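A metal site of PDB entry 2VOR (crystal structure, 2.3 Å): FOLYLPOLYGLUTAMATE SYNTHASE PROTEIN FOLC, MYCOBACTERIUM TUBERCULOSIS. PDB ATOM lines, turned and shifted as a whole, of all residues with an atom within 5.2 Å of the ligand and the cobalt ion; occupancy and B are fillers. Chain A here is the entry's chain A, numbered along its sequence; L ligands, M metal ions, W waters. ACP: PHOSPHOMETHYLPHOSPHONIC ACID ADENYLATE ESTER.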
ATOM      1  N   GLY A  71     -22.284  13.643 -17.800  1.00  0.00           N
ATOM      2  CA  GLY A  71     -20.887  13.334 -18.197  1.00  0.00           C
ATOM      3  C   GLY A  71     -20.039  14.184 -17.302  1.00  0.00           C
ATOM      4  O   GLY A  71     -20.564  14.948 -16.484  1.00  0.00           O
ATOM      5  N   THR A  72     -18.724  14.081 -17.434  1.00  0.00           N
ATOM      6  CA  THR A  72     -17.860  14.862 -16.582  1.00  0.00           C
ATOM      7  C   THR A  72     -17.404  16.144 -17.282  1.00  0.00           C
ATOM      8  O   THR A  72     -17.360  17.237 -16.690  1.00  0.00           O
ATOM      9  CB  THR A  72     -16.566  14.052 -16.166  1.00  0.00           C
ATOM     10  OG1 THR A  72     -16.972  12.828 -15.498  1.00  0.00           O
ATOM     11  CG2 THR A  72     -15.676  14.854 -15.246  1.00  0.00           C
ATOM     12  N   ASN A  73     -17.012  16.013 -18.522  1.00  0.00           N
ATOM     13  CA  ASN A  73     -16.510  17.139 -19.267  1.00  0.00           C
ATOM     14  C   ASN A  73     -17.268  17.339 -20.585  1.00  0.00           C
ATOM     15  O   ASN A  73     -17.581  16.349 -21.303  1.00  0.00           O
ATOM     16  CB  ASN A  73     -15.093  16.899 -19.613  1.00  0.00           C
ATOM     17  CG  ASN A  73     -14.146  17.123 -18.415  1.00  0.00           C
ATOM     18  OD1 ASN A  73     -13.362  16.215 -18.088  1.00  0.00           O
ATOM     19  ND2 ASN A  73     -14.147  18.364 -17.819  1.00  0.00           N
ATOM     20  N   GLY A  74     -17.520  18.623 -20.932  1.00  0.00           N
ATOM     21  CA  GLY A  74     -18.020  18.957 -22.227  1.00  0.00           C
ATOM     22  C   GLY A  74     -19.488  19.029 -22.152  1.00  0.00           C
ATOM     23  O   GLY A  74     -20.091  19.249 -23.129  1.00  0.00           O
ATOM     24  N   LYS A  75     -20.109  18.900 -21.008  1.00  0.00           N
ATOM     25  CA  LYS A  75     -21.558  18.914 -21.072  1.00  0.00           C
ATOM     26  C   LYS A  75     -22.107  20.236 -21.573  1.00  0.00           C
ATOM     27  O   LYS A  75     -23.121  20.285 -22.317  1.00  0.00           O
ATOM     28  CB  LYS A  75     -22.263  18.588 -19.722  1.00  0.00           C
ATOM     29  CG  LYS A  75     -21.779  17.378 -18.928  1.00  0.00           C
ATOM     30  CD  LYS A  75     -22.737  17.184 -17.644  1.00  0.00           C
ATOM     31  CE  LYS A  75     -22.346  18.242 -16.562  1.00  0.00           C
ATOM     32  NZ  LYS A  75     -20.802  18.155 -16.365  1.00  0.00           N
ATOM     33  N   THR A  76     -21.538  21.322 -21.049  1.00  0.00           N
ATOM     34  CA  THR A  76     -21.988  22.691 -21.449  1.00  0.00           C
ATOM     35  C   THR A  76     -21.757  23.009 -22.906  1.00  0.00           C
ATOM     36  O   THR A  76     -22.637  23.430 -23.559  1.00  0.00           O
ATOM     37  CB  THR A  76     -21.404  23.836 -20.583  1.00  0.00           C
ATOM     38  OG1 THR A  76     -22.139  23.850 -19.379  1.00  0.00           O
ATOM     39  CG2 THR A  76     -21.641  25.233 -21.293  1.00  0.00           C
ATOM     40  N   SER A  77     -20.550  22.751 -23.377  1.00  0.00           N
ATOM     41  CA  SER A  77     -20.235  22.825 -24.742  1.00  0.00           C
ATOM     42  C   SER A  77     -21.157  22.060 -25.694  1.00  0.00           C
ATOM     43  O   SER A  77     -21.524  22.615 -26.720  1.00  0.00           O
ATOM     44  CB  SER A  77     -18.843  22.324 -24.953  1.00  0.00           C
ATOM     45  OG  SER A  77     -17.991  23.196 -24.295  1.00  0.00           O
ATOM     46  N   SER A  98     -25.333  24.627 -16.731  1.00  0.00           N
ATOM     47  CA  SER A  98     -24.752  24.981 -15.428  1.00  0.00           C
ATOM     48  C   SER A  98     -23.325  24.565 -15.388  1.00  0.00           C
ATOM     49  O   SER A  98     -22.872  23.791 -16.265  1.00  0.00           O
ATOM     50  CB  SER A  98     -25.509  24.387 -14.226  1.00  0.00           C
ATOM     51  OG  SER A  98     -25.566  22.986 -14.334  1.00  0.00           O
ATOM     52  N   PRO A  99     -22.560  25.171 -14.444  1.00  0.00           N
ATOM     53  CA  PRO A  99     -23.021  26.368 -13.701  1.00  0.00           C
ATOM     54  C   PRO A  99     -22.956  27.651 -14.566  1.00  0.00           C
ATOM     55  O   PRO A  99     -22.375  27.594 -15.642  1.00  0.00           O
ATOM     56  CB  PRO A  99     -21.951  26.533 -12.582  1.00  0.00           C
ATOM     57  CG  PRO A  99     -20.740  25.854 -13.049  1.00  0.00           C
ATOM     58  CD  PRO A  99     -21.116  24.896 -14.268  1.00  0.00           C
ATOM     59  N   GLU A 174     -28.842  20.162 -19.557  1.00  0.00           N
ATOM     60  CA  GLU A 174     -27.668  19.734 -18.850  1.00  0.00           C
ATOM     61  C   GLU A 174     -27.935  19.361 -17.361  1.00  0.00           C
ATOM     62  O   GLU A 174     -28.627  20.059 -16.599  1.00  0.00           O
ATOM     63  CB  GLU A 174     -26.610  20.853 -18.939  1.00  0.00           C
ATOM     64  CG  GLU A 174     -25.381  20.524 -18.230  1.00  0.00           C
ATOM     65  CD  GLU A 174     -24.358  21.641 -18.284  1.00  0.00           C
ATOM     66  OE1 GLU A 174     -24.541  22.707 -18.980  1.00  0.00           O
ATOM     67  OE2 GLU A 174     -23.341  21.428 -17.613  1.00  0.00           O
ATOM     68  N   PRO A 196     -17.578  12.508 -22.104  1.00  0.00           N
ATOM     69  CA  PRO A 196     -16.559  11.713 -21.396  1.00  0.00           C
ATOM     70  C   PRO A 196     -16.623  11.815 -19.857  1.00  0.00           C
ATOM     71  O   PRO A 196     -16.820  12.903 -19.293  1.00  0.00           O
ATOM     72  CB  PRO A 196     -15.266  12.236 -21.966  1.00  0.00           C
ATOM     73  CG  PRO A 196     -15.641  12.639 -23.431  1.00  0.00           C
ATOM     74  CD  PRO A 196     -17.026  13.227 -23.267  1.00  0.00           C
ATOM     75  N   HIS A 297     -10.543  18.283 -28.242  1.00  0.00           N
ATOM     76  CA  HIS A 297     -11.688  17.918 -27.462  1.00  0.00           C
ATOM     77  C   HIS A 297     -13.004  18.518 -27.993  1.00  0.00           C
ATOM     78  O   HIS A 297     -14.075  17.886 -27.885  1.00  0.00           O
ATOM     79  CB  HIS A 297     -11.483  18.251 -25.957  1.00  0.00           C
ATOM     80  CG  HIS A 297     -11.276  19.710 -25.668  1.00  0.00           C
ATOM     81  ND1 HIS A 297     -10.118  20.379 -25.999  1.00  0.00           N
ATOM     82  CD2 HIS A 297     -12.074  20.610 -25.061  1.00  0.00           C
ATOM     83  CE1 HIS A 297     -10.216  21.639 -25.627  1.00  0.00           C
ATOM     84  NE2 HIS A 297     -11.399  21.808 -25.064  1.00  0.00           N
ATOM     85  N   GLN A 298     -12.946  19.708 -28.600  1.00  0.00           N
ATOM     86  CA  GLN A 298     -14.165  20.332 -29.089  1.00  0.00           C
ATOM     87  C   GLN A 298     -14.610  19.642 -30.396  1.00  0.00           C
ATOM     88  O   GLN A 298     -15.764  19.702 -30.742  1.00  0.00           O
ATOM     89  CB  GLN A 298     -14.014  21.884 -29.264  1.00  0.00           C
ATOM     90  CG  GLN A 298     -13.822  22.654 -27.968  1.00  0.00           C
ATOM     91  CD  GLN A 298     -15.090  22.722 -27.140  1.00  0.00           C
ATOM     92  OE1 GLN A 298     -16.053  22.009 -27.380  1.00  0.00           O
ATOM     93  NE2 GLN A 298     -15.096  23.586 -26.138  1.00  0.00           N
ATOM     94  N   ASN A 301     -16.713  16.869 -28.837  1.00  0.00           N
ATOM     95  CA  ASN A 301     -17.992  17.488 -28.467  1.00  0.00           C
ATOM     96  C   ASN A 301     -18.849  17.741 -29.712  1.00  0.00           C
ATOM     97  O   ASN A 301     -20.028  17.410 -29.744  1.00  0.00           O
ATOM     98  CB  ASN A 301     -17.781  18.805 -27.627  1.00  0.00           C
ATOM     99  CG  ASN A 301     -17.108  18.543 -26.255  1.00  0.00           C
ATOM    100  OD1 ASN A 301     -17.215  17.426 -25.738  1.00  0.00           O
ATOM    101  ND2 ASN A 301     -16.447  19.561 -25.670  1.00  0.00           N
ATOM    102  N   SER A 335     -18.930  29.185 -27.012  1.00  0.00           N
ATOM    103  CA  SER A 335     -18.802  28.536 -25.705  1.00  0.00           C
ATOM    104  C   SER A 335     -17.968  29.439 -24.837  1.00  0.00           C
ATOM    105  O   SER A 335     -16.788  29.283 -24.723  1.00  0.00           O
ATOM    106  CB  SER A 335     -18.143  27.160 -25.818  1.00  0.00           C
ATOM    107  OG  SER A 335     -18.398  26.365 -24.629  1.00  0.00           O
ATOM    108  N   GLY A 337     -15.931  31.352 -22.048  1.00  0.00           N
ATOM    109  CA  GLY A 337     -15.049  30.846 -20.972  1.00  0.00           C
ATOM    110  C   GLY A 337     -14.497  29.450 -21.192  1.00  0.00           C
ATOM    111  O   GLY A 337     -13.926  28.857 -20.288  1.00  0.00           O
ATOM    112  N   ARG A 338     -14.695  28.884 -22.373  1.00  0.00           N
ATOM    113  CA  ARG A 338     -13.957  27.660 -22.797  1.00  0.00           C
ATOM    114  C   ARG A 338     -12.950  28.053 -23.912  1.00  0.00           C
ATOM    115  O   ARG A 338     -13.351  28.381 -25.066  1.00  0.00           O
ATOM    116  CB  ARG A 338     -14.922  26.555 -23.279  1.00  0.00           C
ATOM    117  CG  ARG A 338     -15.672  25.814 -22.132  1.00  0.00           C
ATOM    118  CD  ARG A 338     -16.582  26.826 -21.364  1.00  0.00           C
ATOM    119  NE  ARG A 338     -17.544  26.276 -20.395  1.00  0.00           N
ATOM    120  CZ  ARG A 338     -18.441  26.973 -19.682  1.00  0.00           C
ATOM    121  NH1 ARG A 338     -18.589  28.298 -19.825  1.00  0.00           N
ATOM    122  NH2 ARG A 338     -19.237  26.358 -18.817  1.00  0.00           N
ATOM    123  N   LEU A 339     -11.681  28.112 -23.545  1.00  0.00           N
ATOM    124  CA  LEU A 339     -10.596  28.623 -24.408  1.00  0.00           C
ATOM    125  C   LEU A 339     -11.077  29.818 -25.271  1.00  0.00           C
ATOM    126  O   LEU A 339     -11.048  29.793 -26.516  1.00  0.00           O
ATOM    127  CB  LEU A 339     -10.138  27.510 -25.292  1.00  0.00           C
ATOM    128  CG  LEU A 339      -8.667  27.081 -25.364  1.00  0.00           C
ATOM    129  CD1 LEU A 339      -7.779  27.991 -24.625  1.00  0.00           C
ATOM    130  CD2 LEU A 339      -8.572  25.616 -24.940  1.00  0.00           C
ATOM    131  N   ASP A 351     -10.201  29.993 -19.632  1.00  0.00           N
ATOM    132  CA  ASP A 351     -10.693  28.632 -19.820  1.00  0.00           C
ATOM    133  C   ASP A 351     -11.170  28.033 -18.535  1.00  0.00           C
ATOM    134  O   ASP A 351     -10.544  28.183 -17.535  1.00  0.00           O
ATOM    135  CB  ASP A 351      -9.685  27.727 -20.499  1.00  0.00           C
ATOM    136  CG  ASP A 351     -10.265  26.308 -20.750  1.00  0.00           C
ATOM    137  OD1 ASP A 351     -11.034  26.087 -21.711  1.00  0.00           O
ATOM    138  OD2 ASP A 351      -9.982  25.400 -19.933  1.00  0.00           O
ATOM    139  N   ALA A 352     -12.312  27.357 -18.543  1.00  0.00           N
ATOM    140  CA  ALA A 352     -12.971  26.954 -17.306  1.00  0.00           C
ATOM    141  C   ALA A 352     -12.436  25.632 -16.790  1.00  0.00           C
ATOM    142  O   ALA A 352     -13.123  24.986 -16.002  1.00  0.00           O
ATOM    143  CB  ALA A 352     -14.569  26.848 -17.551  1.00  0.00           C
ATOM    144  N   ALA A 353     -11.255  25.193 -17.238  1.00  0.00           N
ATOM    145  CA  ALA A 353     -10.678  23.865 -16.850  1.00  0.00           C
ATOM    146  C   ALA A 353     -10.566  23.699 -15.343  1.00  0.00           C
ATOM    147  O   ALA A 353      -9.897  24.460 -14.688  1.00  0.00           O
ATOM    148  CB  ALA A 353      -9.311  23.651 -17.499  1.00  0.00           C
ATOM    149  N   HIS A 354     -11.240  22.721 -14.779  1.00  0.00           N
ATOM    150  CA  HIS A 354     -11.249  22.563 -13.335  1.00  0.00           C
ATOM    151  C   HIS A 354     -11.076  21.112 -12.890  1.00  0.00           C
ATOM    152  O   HIS A 354     -11.427  20.749 -11.782  1.00  0.00           O
ATOM    153  CB  HIS A 354     -12.480  23.192 -12.691  1.00  0.00           C
ATOM    154  CG  HIS A 354     -13.793  22.713 -13.231  1.00  0.00           C
ATOM    155  ND1 HIS A 354     -14.371  21.508 -12.847  1.00  0.00           N
ATOM    156  CD2 HIS A 354     -14.693  23.313 -14.052  1.00  0.00           C
ATOM    157  CE1 HIS A 354     -15.548  21.381 -13.436  1.00  0.00           C
ATOM    158  NE2 HIS A 354     -15.740  22.451 -14.198  1.00  0.00           N
ATOM    159  N   ALA A 357      -8.503  16.002 -16.544  1.00  0.00           N
ATOM    160  CA  ALA A 357      -8.797  15.744 -17.938  1.00  0.00           C
ATOM    161  C   ALA A 357      -9.012  17.079 -18.670  1.00  0.00           C
ATOM    162  O   ALA A 357      -8.499  17.265 -19.764  1.00  0.00           O
ATOM    163  CB  ALA A 357     -10.040  14.852 -18.040  1.00  0.00           C
ATOM    164  N   GLY A 358      -9.725  18.020 -18.076  1.00  0.00           N
ATOM    165  CA  GLY A 358      -9.958  19.381 -18.670  1.00  0.00           C
ATOM    166  C   GLY A 358      -8.652  20.179 -18.777  1.00  0.00           C
ATOM    167  O   GLY A 358      -8.371  20.798 -19.790  1.00  0.00           O
ATOM    168  N   ALA A 359      -7.872  20.158 -17.728  1.00  0.00           N
ATOM    169  CA  ALA A 359      -6.537  20.802 -17.614  1.00  0.00           C
ATOM    170  C   ALA A 359      -5.546  20.251 -18.680  1.00  0.00           C
ATOM    171  O   ALA A 359      -4.710  20.961 -19.304  1.00  0.00           O
ATOM    172  CB  ALA A 359      -6.003  20.551 -16.169  1.00  0.00           C
ATOM    173  N   ALA A 361      -6.537  18.759 -21.497  1.00  0.00           N
ATOM    174  CA  ALA A 361      -7.086  19.140 -22.810  1.00  0.00           C
ATOM    175  C   ALA A 361      -6.723  20.598 -23.088  1.00  0.00           C
ATOM    176  O   ALA A 361      -6.302  20.940 -24.182  1.00  0.00           O
ATOM    177  CB  ALA A 361      -8.631  18.896 -22.879  1.00  0.00           C
ATOM    178  N   LEU A 362      -6.806  21.448 -22.064  1.00  0.00           N
ATOM    179  CA  LEU A 362      -6.300  22.783 -22.202  1.00  0.00           C
ATOM    180  C   LEU A 362      -4.787  22.853 -22.596  1.00  0.00           C
ATOM    181  O   LEU A 362      -4.449  23.573 -23.506  1.00  0.00           O
ATOM    182  CB  LEU A 362      -6.597  23.580 -20.928  1.00  0.00           C
ATOM    183  CG  LEU A 362      -5.900  24.954 -20.873  1.00  0.00           C
ATOM    184  CD1 LEU A 362      -6.556  25.780 -22.010  1.00  0.00           C
ATOM    185  CD2 LEU A 362      -5.987  25.684 -19.476  1.00  0.00           C
ATOM    186  N   VAL A 472     -14.739  27.549 -13.279  1.00  0.00           N
ATOM    187  CA  VAL A 472     -15.798  28.245 -13.960  1.00  0.00           C
ATOM    188  C   VAL A 472     -15.936  29.625 -13.383  1.00  0.00           C
ATOM    189  O   VAL A 472     -16.201  30.608 -14.122  1.00  0.00           O
ATOM    190  CB  VAL A 472     -17.131  27.570 -13.692  1.00  0.00           C
ATOM    191  CG1 VAL A 472     -18.296  28.441 -14.175  1.00  0.00           C
ATOM    192  CG2 VAL A 472     -17.140  26.248 -14.358  1.00  0.00           C
HETATM  193  PG  ACP L   1     -18.544  22.918 -16.224  1.00  0.00           P
HETATM  194  O1G ACP L   1     -19.759  23.583 -17.388  1.00  0.00           O
HETATM  195  O2G ACP L   1     -18.938  22.732 -14.743  1.00  0.00           O
HETATM  196  O3G ACP L   1     -17.326  23.767 -16.431  1.00  0.00           O
HETATM  197  PB  ACP L   1     -18.850  20.767 -18.335  1.00  0.00           P
HETATM  198  O1B ACP L   1     -18.966  19.295 -18.264  1.00  0.00           O
HETATM  199  O2B ACP L   1     -20.192  21.355 -18.554  1.00  0.00           O
HETATM  200  C3B ACP L   1     -18.479  21.128 -16.563  1.00  0.00           C
HETATM  201  PA  ACP L   1     -17.846  22.330 -20.359  1.00  0.00           P
HETATM  202  O1A ACP L   1     -17.831  23.701 -19.573  1.00  0.00           O
HETATM  203  O2A ACP L   1     -17.658  22.322 -21.856  1.00  0.00           O
HETATM  204  O3A ACP L   1     -17.668  21.053 -19.321  1.00  0.00           O
HETATM  205  O5' ACP L   1     -16.124  22.395 -20.304  1.00  0.00           O
HETATM  206  C5' ACP L   1     -15.291  22.638 -19.078  1.00  0.00           C
HETATM  207  C4' ACP L   1     -13.808  22.576 -19.365  1.00  0.00           C
HETATM  208  O4' ACP L   1     -13.604  21.188 -19.721  1.00  0.00           O
HETATM  209  C3' ACP L   1     -13.496  23.308 -20.668  1.00  0.00           C
HETATM  210  O3' ACP L   1     -13.062  24.639 -20.454  1.00  0.00           O
HETATM  211  C2' ACP L   1     -12.360  22.510 -21.301  1.00  0.00           C
HETATM  212  O2' ACP L   1     -11.098  22.819 -20.705  1.00  0.00           O
HETATM  213  C1' ACP L   1     -12.667  21.104 -20.852  1.00  0.00           C
HETATM  214  N9  ACP L   1     -13.415  20.201 -21.775  1.00  0.00           N
HETATM  215  C8  ACP L   1     -14.595  20.426 -22.439  1.00  0.00           C
HETATM  216  N7  ACP L   1     -14.959  19.324 -23.127  1.00  0.00           N
HETATM  217  C5  ACP L   1     -13.982  18.418 -22.918  1.00  0.00           C
HETATM  218  C6  ACP L   1     -13.801  17.115 -23.336  1.00  0.00           C
HETATM  219  N6  ACP L   1     -14.685  16.530 -24.143  1.00  0.00           N
HETATM  220  N1  ACP L   1     -12.723  16.468 -22.889  1.00  0.00           N
HETATM  221  C2  ACP L   1     -11.805  17.033 -22.120  1.00  0.00           C
HETATM  222  N3  ACP L   1     -11.942  18.276 -21.687  1.00  0.00           N
HETATM  223  C4  ACP L   1     -13.027  18.960 -22.056  1.00  0.00           C
HETATM  224 CO    CO M   1     -21.484  22.639 -17.451  1.00  0.00          CO
HETATM  225  O   HOH W   1     -12.751  20.888 -16.628  1.00  0.00           O
HETATM  226  O   HOH W   2     -16.055  19.990 -15.933  1.00  0.00           O
HETATM  227  O   HOH W   3     -12.454  24.230 -24.347  1.00  0.00           O
HETATM  228  O   HOH W   4     -11.870  13.687 -22.703  1.00  0.00           O
HETATM  229  O   HOH W   5     -12.781  14.354 -25.883  1.00  0.00           O
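The side-chain hydroxyl of Ser 77 lies within hydrogen-bond range of an oxygen (O2A) of the ligand. The backbone NH of Lys 75 is in hydrogen-bond range of an oxygen (O1B) of the ligand (3.0 Å). O2A of the ligand is in hydrogen-bond range of N of Ser 77 (3.3 Å). OD1 of Asp 351 sits at hydrogen-bond distance from O3' of the ligand, at 2.8 Å. A nitrogen (N7) of the ligand is in hydrogen-bond range of the side-chain amide nitrogen of Asn 301. An oxygen (O3G) of the ligand sits at hydrogen-bond distance from a ring nitrogen (NE2) of His 354, at 3.0 Å. An oxygen (O1B) of the ligand lies close to the backbone carbonyl oxygen (O) of Thr 72, 3.0 Å away. NE of Arg 338 is in salt-bridge range of O1A of the ligand (2.7 Å). O4' of the ligand sits at hydrogen-bond distance from ND2 of Asn 73, at 3.4 Å. An oxygen (O3A) of the ligand lies within hydrogen-bond range of the backbone NH (N) of Gly 74 (2.9 Å). O2B of the ligand lies close to N of Thr 76, at 2.8 Å. N of Ala 352 is in hydrogen-bond range of O3' of the ligand, at 3.4 Å. NZ of Lys 75 lies within salt-bridge range of O1B of the ligand, 2.9 Å away.
N of Leu 339 lies within hydrogen-bond range of OD1 of Asp 351, at 2.8 Å. The backbone NH (N) of Ala 352 is in hydrogen-bond range of the backbone carbonyl oxygen (O) of Gly 337, 2.8 Å away. The side-chain amide oxygen (OE1) of Gln 298 is in hydrogen-bond range of the side-chain amide nitrogen (ND2) of Asn 301 (3.0 Å). The backbone NH (N) of Asn 73 is in hydrogen-bond range of the backbone carbonyl oxygen (O) of Pro 196 (3.2 Å). The side-chain hydroxyl (OG) of Ser 77 lies within hydrogen-bond range of the side-chain amide nitrogen (NE2) of Gln 298, at 3.5 Å. The backbone NH (N) of Thr 72 sits at hydrogen-bond distance from the backbone carbonyl oxygen (O) of Pro 196 (2.9 Å). The side-chain hydroxyl (OG) of Ser 77 is in hydrogen-bond range of the side-chain hydroxyl (OG) of Ser 335 (3.2 Å). OD2 of Asp 351 sits at hydrogen-bond distance from N of Ala 353 (3.0 Å).
CD of Pro 99 touches O2G of the ligand, 3.1 Å away. His 297 touches the ligand (CD2 to C4, 3.6 Å). Ala 353 touches the ligand (N to O3', 3.7 Å). Gly 358 touches the ligand. Ala 361 touches the ligand. CG2 of Val 472 touches O3G of the ligand, at 3.2 Å. Hydrophobic or aromatic side chains that line the ligand: Pro 99, His 297, Ala 352, Ala 353, His 354, Ala 361 and Val 472. 19 residues have an atom within 4 Å of the ligand: Thr 72, Asn 73, Gly 74, Lys 75, Thr 76, Ser 77, Ser 98, Pro 99, Glu 174, His 297, Asn 301, Arg 338, Asp 351, Ala 352, Ala 353, His 354, Gly 358, Ala 361 and Val 472.
Residues that only touch the cobalt ion: Pro 99. The nearest printed residue that does not touch the cobalt ion is Arg 338 (4.6 Å).
The cobalt ion is bound by an oxygen (O1G) of the ligand (2.0 Å), an oxygen (O2B) of the ligand (2.1 Å), the backbone carbonyl oxygen of Ser 98 (2.2 Å), the side-chain carboxylate of Glu 174 (2.2 Å) and the side-chain hydroxyl of Thr 76 (2.4 Å).
Water W2 lies within hydrogen-bond range of NE2 of His 354 (3.0 Å), ND2 of Asn 73 (3.1 Å) and O of Thr 72 (3.1 Å). Water W1 lies within hydrogen-bond range of the backbone NH of His 354 (3.0 Å), the side-chain amide nitrogen of Asn 73 (3.1 Å) and an oxygen (O4') of the ligand (3.2 Å). Water W3 lies within hydrogen-bond range of NE2 of His 297 and NE2 of Gln 298.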
